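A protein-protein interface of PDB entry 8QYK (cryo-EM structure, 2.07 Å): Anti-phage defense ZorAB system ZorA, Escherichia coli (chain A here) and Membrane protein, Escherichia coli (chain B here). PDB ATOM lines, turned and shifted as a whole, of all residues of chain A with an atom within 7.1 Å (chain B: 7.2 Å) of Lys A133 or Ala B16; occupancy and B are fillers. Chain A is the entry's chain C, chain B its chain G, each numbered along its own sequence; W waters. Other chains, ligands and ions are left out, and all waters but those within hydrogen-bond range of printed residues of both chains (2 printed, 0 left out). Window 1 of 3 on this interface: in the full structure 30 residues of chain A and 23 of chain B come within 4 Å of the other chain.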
ATOM      1  N   TYR A  38      10.929  25.653   8.783  1.00  0.00           N
ATOM      2  CA  TYR A  38      12.161  24.893   8.947  1.00  0.00           C
ATOM      3  C   TYR A  38      12.165  23.619   8.114  1.00  0.00           C
ATOM      4  O   TYR A  38      13.051  23.448   7.272  1.00  0.00           O
ATOM      5  CB  TYR A  38      12.372  24.575  10.433  1.00  0.00           C
ATOM      6  CG  TYR A  38      13.697  23.925  10.752  1.00  0.00           C
ATOM      7  CD1 TYR A  38      13.866  22.552  10.643  1.00  0.00           C
ATOM      8  CD2 TYR A  38      14.781  24.685  11.168  1.00  0.00           C
ATOM      9  CE1 TYR A  38      15.071  21.956  10.934  1.00  0.00           C
ATOM     10  CE2 TYR A  38      15.991  24.098  11.461  1.00  0.00           C
ATOM     11  CZ  TYR A  38      16.131  22.731  11.343  1.00  0.00           C
ATOM     12  OH  TYR A  38      17.334  22.138  11.637  1.00  0.00           O
ATOM     13  N   ASP A 124      22.209  27.363   8.158  1.00  0.00           N
ATOM     14  CA  ASP A 124      21.907  27.848   9.503  1.00  0.00           C
ATOM     15  C   ASP A 124      21.052  29.110   9.481  1.00  0.00           C
ATOM     16  O   ASP A 124      20.077  29.217  10.232  1.00  0.00           O
ATOM     17  CB  ASP A 124      23.204  28.099  10.267  1.00  0.00           C
ATOM     18  CG  ASP A 124      23.982  26.827  10.524  1.00  0.00           C
ATOM     19  OD1 ASP A 124      25.223  26.858  10.420  1.00  0.00           O
ATOM     20  OD2 ASP A 124      23.356  25.795  10.837  1.00  0.00           O
ATOM     21  N   ASN A 128      16.992  29.425  10.064  1.00  0.00           N
ATOM     22  CA  ASN A 128      16.815  30.097  11.350  1.00  0.00           C
ATOM     23  C   ASN A 128      17.081  29.143  12.509  1.00  0.00           C
ATOM     24  O   ASN A 128      16.300  29.049  13.457  1.00  0.00           O
ATOM     25  CB  ASN A 128      15.424  30.722  11.465  1.00  0.00           C
ATOM     26  CG  ASN A 128      15.245  31.918  10.557  1.00  0.00           C
ATOM     27  OD1 ASN A 128      15.718  33.013  10.855  1.00  0.00           O
ATOM     28  ND2 ASN A 128      14.560  31.715   9.442  1.00  0.00           N
ATOM     29  N   THR A 129      18.200  28.420  12.428  1.00  0.00           N
ATOM     30  CA  THR A 129      18.556  27.483  13.487  1.00  0.00           C
ATOM     31  C   THR A 129      18.820  28.182  14.814  1.00  0.00           C
ATOM     32  O   THR A 129      18.576  27.589  15.867  1.00  0.00           O
ATOM     33  CB  THR A 129      19.785  26.664  13.090  1.00  0.00           C
ATOM     34  OG1 THR A 129      20.944  27.506  13.079  1.00  0.00           O
ATOM     35  CG2 THR A 129      19.598  26.042  11.718  1.00  0.00           C
ATOM     36  N   GLU A 130      19.303  29.428  14.787  1.00  0.00           N
ATOM     37  CA  GLU A 130      19.541  30.164  16.023  1.00  0.00           C
ATOM     38  C   GLU A 130      18.276  30.321  16.854  1.00  0.00           C
ATOM     39  O   GLU A 130      18.367  30.479  18.075  1.00  0.00           O
ATOM     40  CB  GLU A 130      20.135  31.538  15.719  1.00  0.00           C
ATOM     41  CG  GLU A 130      21.599  31.510  15.329  1.00  0.00           C
ATOM     42  CD  GLU A 130      22.484  30.952  16.425  1.00  0.00           C
ATOM     43  OE1 GLU A 130      22.739  31.673  17.410  1.00  0.00           O
ATOM     44  OE2 GLU A 130      22.933  29.795  16.296  1.00  0.00           O
ATOM     45  N   PHE A 131      17.106  30.284  16.225  1.00  0.00           N
ATOM     46  CA  PHE A 131      15.843  30.263  16.945  1.00  0.00           C
ATOM     47  C   PHE A 131      15.320  28.853  17.175  1.00  0.00           C
ATOM     48  O   PHE A 131      14.998  28.497  18.313  1.00  0.00           O
ATOM     49  CB  PHE A 131      14.783  31.070  16.188  1.00  0.00           C
ATOM     50  CG  PHE A 131      13.390  30.869  16.710  1.00  0.00           C
ATOM     51  CD1 PHE A 131      12.959  31.544  17.838  1.00  0.00           C
ATOM     52  CD2 PHE A 131      12.518  29.990  16.085  1.00  0.00           C
ATOM     53  CE1 PHE A 131      11.682  31.353  18.330  1.00  0.00           C
ATOM     54  CE2 PHE A 131      11.242  29.796  16.570  1.00  0.00           C
ATOM     55  CZ  PHE A 131      10.821  30.479  17.694  1.00  0.00           C
ATOM     56  N   PHE A 132      15.247  28.038  16.123  1.00  0.00           N
ATOM     57  CA  PHE A 132      14.508  26.783  16.175  1.00  0.00           C
ATOM     58  C   PHE A 132      15.162  25.712  17.039  1.00  0.00           C
ATOM     59  O   PHE A 132      14.466  24.788  17.465  1.00  0.00           O
ATOM     60  CB  PHE A 132      14.292  26.241  14.762  1.00  0.00           C
ATOM     61  CG  PHE A 132      13.093  26.820  14.078  1.00  0.00           C
ATOM     62  CD1 PHE A 132      11.815  26.501  14.504  1.00  0.00           C
ATOM     63  CD2 PHE A 132      13.242  27.698  13.020  1.00  0.00           C
ATOM     64  CE1 PHE A 132      10.711  27.044  13.883  1.00  0.00           C
ATOM     65  CE2 PHE A 132      12.142  28.235  12.390  1.00  0.00           C
ATOM     66  CZ  PHE A 132      10.877  27.914  12.823  1.00  0.00           C
ATOM     67  N   LYS A 133      16.464  25.800  17.312  1.00  0.00           N
ATOM     68  CA  LYS A 133      17.057  24.827  18.222  1.00  0.00           C
ATOM     69  C   LYS A 133      16.549  24.991  19.649  1.00  0.00           C
ATOM     70  O   LYS A 133      16.692  24.066  20.453  1.00  0.00           O
ATOM     71  CB  LYS A 133      18.585  24.910  18.203  1.00  0.00           C
ATOM     72  CG  LYS A 133      19.165  26.207  18.719  1.00  0.00           C
ATOM     73  CD  LYS A 133      20.685  26.167  18.681  1.00  0.00           C
ATOM     74  CE  LYS A 133      21.215  26.272  17.264  1.00  0.00           C
ATOM     75  NZ  LYS A 133      22.699  26.363  17.244  1.00  0.00           N
ATOM     76  N   HIS A 134      15.954  26.134  19.972  1.00  0.00           N
ATOM     77  CA  HIS A 134      15.377  26.382  21.284  1.00  0.00           C
ATOM     78  C   HIS A 134      13.874  26.139  21.335  1.00  0.00           C
ATOM     79  O   HIS A 134      13.275  26.281  22.403  1.00  0.00           O
ATOM     80  CB  HIS A 134      15.690  27.816  21.728  1.00  0.00           C
ATOM     81  CG  HIS A 134      17.153  28.124  21.775  1.00  0.00           C
ATOM     82  ND1 HIS A 134      17.937  27.833  22.869  1.00  0.00           N
ATOM     83  CD2 HIS A 134      17.980  28.680  20.858  1.00  0.00           C
ATOM     84  CE1 HIS A 134      19.181  28.201  22.629  1.00  0.00           C
ATOM     85  NE2 HIS A 134      19.236  28.718  21.416  1.00  0.00           N
ATOM     86  N   LEU A 135      13.257  25.770  20.212  1.00  0.00           N
ATOM     87  CA  LEU A 135      11.811  25.555  20.193  1.00  0.00           C
ATOM     88  C   LEU A 135      11.328  24.415  21.089  1.00  0.00           C
ATOM     89  O   LEU A 135      10.305  24.604  21.770  1.00  0.00           O
ATOM     90  CB  LEU A 135      11.339  25.344  18.748  1.00  0.00           C
ATOM     91  CG  LEU A 135       9.827  25.188  18.563  1.00  0.00           C
ATOM     92  CD1 LEU A 135       9.078  26.398  19.108  1.00  0.00           C
ATOM     93  CD2 LEU A 135       9.478  24.955  17.108  1.00  0.00           C
ATOM     94  N   PRO A 136      11.956  23.229  21.119  1.00  0.00           N
ATOM     95  CA  PRO A 136      11.426  22.158  21.988  1.00  0.00           C
ATOM     96  C   PRO A 136      11.352  22.542  23.456  1.00  0.00           C
ATOM     97  O   PRO A 136      10.396  22.163  24.152  1.00  0.00           O
ATOM     98  CB  PRO A 136      12.409  21.002  21.749  1.00  0.00           C
ATOM     99  CG  PRO A 136      12.984  21.269  20.417  1.00  0.00           C
ATOM    100  CD  PRO A 136      13.089  22.750  20.306  1.00  0.00           C
ATOM    101  N   GLY A 137      12.334  23.301  23.944  1.00  0.00           N
ATOM    102  CA  GLY A 137      12.258  23.803  25.305  1.00  0.00           C
ATOM    103  C   GLY A 137      11.075  24.728  25.506  1.00  0.00           C
ATOM    104  O   GLY A 137      10.407  24.680  26.540  1.00  0.00           O
ATOM    105  N   THR A 195      12.398  17.927  17.892  1.00  0.00           N
ATOM    106  CA  THR A 195      13.823  17.646  18.038  1.00  0.00           C
ATOM    107  C   THR A 195      14.280  16.605  17.028  1.00  0.00           C
ATOM    108  O   THR A 195      15.289  16.792  16.339  1.00  0.00           O
ATOM    109  CB  THR A 195      14.128  17.170  19.458  1.00  0.00           C
ATOM    110  OG1 THR A 195      13.629  18.120  20.403  1.00  0.00           O
ATOM    111  CG2 THR A 195      15.628  17.006  19.651  1.00  0.00           C
ATOM    112  N   GLU A 198      14.131  18.117  13.421  1.00  0.00           N
ATOM    113  CA  GLU A 198      15.089  19.197  13.234  1.00  0.00           C
ATOM    114  C   GLU A 198      16.514  18.668  13.183  1.00  0.00           C
ATOM    115  O   GLU A 198      17.302  19.065  12.319  1.00  0.00           O
ATOM    116  CB  GLU A 198      14.933  20.221  14.358  1.00  0.00           C
ATOM    117  CG  GLU A 198      16.068  21.215  14.448  1.00  0.00           C
ATOM    118  CD  GLU A 198      16.309  21.708  15.858  1.00  0.00           C
ATOM    119  OE1 GLU A 198      15.627  21.232  16.788  1.00  0.00           O
ATOM    120  OE2 GLU A 198      17.193  22.569  16.039  1.00  0.00           O
ATOM    121  N   LYS A 199      16.867  17.767  14.102  1.00  0.00           N
ATOM    122  CA  LYS A 199      18.232  17.265  14.146  1.00  0.00           C
ATOM    123  C   LYS A 199      18.526  16.362  12.957  1.00  0.00           C
ATOM    124  O   LYS A 199      19.622  16.420  12.387  1.00  0.00           O
ATOM    125  CB  LYS A 199      18.481  16.540  15.466  1.00  0.00           C
ATOM    126  CG  LYS A 199      18.455  17.462  16.678  1.00  0.00           C
ATOM    127  CD  LYS A 199      19.384  18.651  16.485  1.00  0.00           C
ATOM    128  CE  LYS A 199      18.854  19.904  17.155  1.00  0.00           C
ATOM    129  NZ  LYS A 199      18.680  19.748  18.618  1.00  0.00           N
ATOM    130  N   TYR A 206      23.886  19.109   6.491  1.00  0.00           N
ATOM    131  CA  TYR A 206      25.343  19.171   6.550  1.00  0.00           C
ATOM    132  C   TYR A 206      25.979  18.095   5.675  1.00  0.00           C
ATOM    133  O   TYR A 206      26.956  18.363   4.968  1.00  0.00           O
ATOM    134  CB  TYR A 206      25.819  19.053   7.997  1.00  0.00           C
ATOM    135  CG  TYR A 206      25.519  20.277   8.834  1.00  0.00           C
ATOM    136  CD1 TYR A 206      24.932  21.401   8.272  1.00  0.00           C
ATOM    137  CD2 TYR A 206      25.816  20.305  10.189  1.00  0.00           C
ATOM    138  CE1 TYR A 206      24.652  22.517   9.027  1.00  0.00           C
ATOM    139  CE2 TYR A 206      25.539  21.421  10.956  1.00  0.00           C
ATOM    140  CZ  TYR A 206      24.957  22.522  10.368  1.00  0.00           C
ATOM    141  OH  TYR A 206      24.676  23.636  11.119  1.00  0.00           O
ATOM    142  N   ARG B  11      30.040  30.532  13.946  1.00  0.00           N
ATOM    143  CA  ARG B  11      29.771  31.251  15.220  1.00  0.00           C
ATOM    144  C   ARG B  11      29.665  30.312  16.432  1.00  0.00           C
ATOM    145  O   ARG B  11      29.298  29.154  16.252  1.00  0.00           O
ATOM    146  CB  ARG B  11      28.472  32.050  15.070  1.00  0.00           C
ATOM    147  CG  ARG B  11      27.306  31.663  15.966  1.00  0.00           C
ATOM    148  CD  ARG B  11      25.968  31.806  15.268  1.00  0.00           C
ATOM    149  NE  ARG B  11      25.974  32.735  14.144  1.00  0.00           N
ATOM    150  CZ  ARG B  11      25.154  32.666  13.099  1.00  0.00           C
ATOM    151  NH1 ARG B  11      25.269  33.533  12.112  1.00  0.00           N
ATOM    152  NH2 ARG B  11      24.216  31.736  13.039  1.00  0.00           N
ATOM    153  N   ARG B  12      29.988  30.813  17.623  1.00  0.00           N
ATOM    154  CA  ARG B  12      29.844  30.073  18.895  1.00  0.00           C
ATOM    155  C   ARG B  12      28.332  29.983  19.104  1.00  0.00           C
ATOM    156  O   ARG B  12      27.679  31.027  19.282  1.00  0.00           O
ATOM    157  CB  ARG B  12      30.663  30.855  19.931  1.00  0.00           C
ATOM    158  CG  ARG B  12      32.172  30.863  19.719  1.00  0.00           C
ATOM    159  CD  ARG B  12      32.954  31.681  20.729  1.00  0.00           C
ATOM    160  NE  ARG B  12      34.395  31.655  20.522  1.00  0.00           N
ATOM    161  CZ  ARG B  12      35.040  32.433  19.663  1.00  0.00           C
ATOM    162  NH1 ARG B  12      34.656  33.688  19.497  1.00  0.00           N
ATOM    163  NH2 ARG B  12      36.057  31.951  18.970  1.00  0.00           N
ATOM    164  N   SER B  13      27.771  28.799  18.963  1.00  0.00           N
ATOM    165  CA  SER B  13      26.295  28.640  18.993  1.00  0.00           C
ATOM    166  C   SER B  13      25.823  28.296  20.396  1.00  0.00           C
ATOM    167  O   SER B  13      26.062  27.152  20.825  1.00  0.00           O
ATOM    168  CB  SER B  13      25.844  27.644  17.969  1.00  0.00           C
ATOM    169  OG  SER B  13      24.439  27.470  18.043  1.00  0.00           O
ATOM    170  N   ASP B  14      25.198  29.254  21.077  1.00  0.00           N
ATOM    171  CA  ASP B  14      24.590  28.967  22.396  1.00  0.00           C
ATOM    172  C   ASP B  14      23.905  27.611  22.307  1.00  0.00           C
ATOM    173  O   ASP B  14      23.155  27.352  21.349  1.00  0.00           O
ATOM    174  CB  ASP B  14      23.498  29.951  22.823  1.00  0.00           C
ATOM    175  CG  ASP B  14      22.937  29.631  24.204  1.00  0.00           C
ATOM    176  OD1 ASP B  14      21.750  29.898  24.447  1.00  0.00           O
ATOM    177  OD2 ASP B  14      23.699  29.109  25.035  1.00  0.00           O
ATOM    178  N   GLU B  15      24.144  26.796  23.308  1.00  0.00           N
ATOM    179  CA  GLU B  15      23.518  25.472  23.275  1.00  0.00           C
ATOM    180  C   GLU B  15      22.231  25.585  24.088  1.00  0.00           C
ATOM    181  O   GLU B  15      22.224  26.289  25.090  1.00  0.00           O
ATOM    182  CB  GLU B  15      24.539  24.386  23.626  1.00  0.00           C
ATOM    183  CG  GLU B  15      25.621  24.246  22.566  1.00  0.00           C
ATOM    184  CD  GLU B  15      26.720  23.236  22.868  1.00  0.00           C
ATOM    185  OE1 GLU B  15      26.767  22.745  24.014  1.00  0.00           O
ATOM    186  OE2 GLU B  15      27.521  22.923  21.958  1.00  0.00           O
ATOM    187  N   ALA B  16      21.184  24.930  23.633  1.00  0.00           N
ATOM    188  CA  ALA B  16      19.854  25.024  24.250  1.00  0.00           C
ATOM    189  C   ALA B  16      19.698  24.294  25.572  1.00  0.00           C
ATOM    190  O   ALA B  16      20.506  23.456  25.889  1.00  0.00           O
ATOM    191  CB  ALA B  16      18.881  24.456  23.244  1.00  0.00           C
ATOM    192  N   GLU B  17      18.577  24.544  26.202  1.00  0.00           N
ATOM    193  CA  GLU B  17      18.239  23.825  27.448  1.00  0.00           C
ATOM    194  C   GLU B  17      18.022  22.364  27.074  1.00  0.00           C
ATOM    195  O   GLU B  17      17.223  22.106  26.174  1.00  0.00           O
ATOM    196  CB  GLU B  17      17.055  24.536  28.098  1.00  0.00           C
ATOM    197  CG  GLU B  17      16.546  23.893  29.372  1.00  0.00           C
ATOM    198  CD  GLU B  17      17.547  23.721  30.502  1.00  0.00           C
ATOM    199  OE1 GLU B  17      17.909  24.733  31.123  1.00  0.00           O
ATOM    200  OE2 GLU B  17      17.945  22.568  30.768  1.00  0.00           O
ATOM    201  N   LYS B  18      18.771  21.459  27.693  1.00  0.00           N
ATOM    202  CA  LYS B  18      18.549  20.028  27.514  1.00  0.00           C
ATOM    203  C   LYS B  18      17.079  19.720  27.748  1.00  0.00           C
ATOM    204  O   LYS B  18      16.517  20.168  28.754  1.00  0.00           O
ATOM    205  CB  LYS B  18      19.421  19.212  28.459  1.00  0.00           C
ATOM    206  CG  LYS B  18      20.900  19.483  28.322  1.00  0.00           C
ATOM    207  CD  LYS B  18      21.704  18.566  29.217  1.00  0.00           C
ATOM    208  CE  LYS B  18      21.533  17.115  28.815  1.00  0.00           C
ATOM    209  NZ  LYS B  18      22.362  16.188  29.631  1.00  0.00           N
ATOM    210  N   PRO B  19      16.414  19.006  26.840  1.00  0.00           N
ATOM    211  CA  PRO B  19      14.983  18.726  27.031  1.00  0.00           C
ATOM    212  C   PRO B  19      14.680  17.938  28.287  1.00  0.00           C
ATOM    213  O   PRO B  19      13.576  18.075  28.838  1.00  0.00           O
ATOM    214  CB  PRO B  19      14.612  17.930  25.774  1.00  0.00           C
ATOM    215  CG  PRO B  19      15.907  17.323  25.317  1.00  0.00           C
ATOM    216  CD  PRO B  19      16.963  18.331  25.652  1.00  0.00           C
HETATM  217  O   HOH W   1      16.903  27.335  25.106  1.00  0.00           O
HETATM  218  O   HOH W   2      25.836  29.093  12.660  1.00  0.00           O
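Hydrophobic or aromatic side chains of chain A that line the printed part of chain B: His A134. Along chain A the printed residues that touch a printed residue of chain B span positions 130 to 134. Of the 9 printed residues of chain B, 4 touch a printed residue of chain A. Among the printed residues, 7 pairs touch across the chains.
Water W1 lies within hydrogen-bond range of ND1 of His A134 and N of Glu B17. Water W2 lies within hydrogen-bond range of the guanidinium group of Arg B11 (3.1 Å) and the side-chain carboxylate of Asp A124 (3.2 Å).
Lys A133 touches three residues of chain B. Ala B16 touches just these residues of chain A: Lys A133 and His A134. Printed residues of chain B within 4 Å of Glu A130: Arg B11 and Ser B13. Printed residues of chain A within 4 Å of Ser B13: Glu A130 and Lys A133. Of the printed residues of chain B, His A134 touches Asp B14 (3.6 Å) and Ala B16 (3.5 Å). The nearest residue of chain A that does not touch Ala B16 is Leu A135 (6.5 Å).
Among the printed residues, merely in contact across the chains: Glu A130 with Arg B11 (3.5 Å), His A134 with Ala B16 (3.5 Å), Lys A133 with Ala B16 (3.6 Å), His A134 with Asp B14 (3.6 Å) and Lys A133 with Asp B14 (3.8 Å).
OE2 of Glu A130 is in hydrogen-bond range of OG of Ser B13 (3.3 Å). NZ of Lys A133 lies close to OG of Ser B13, at 2.2 Å.
The side-chain amino group (NZ) of Lys A133 lies within salt-bridge range of the side-chain carboxylate (OE2) of Glu A130.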
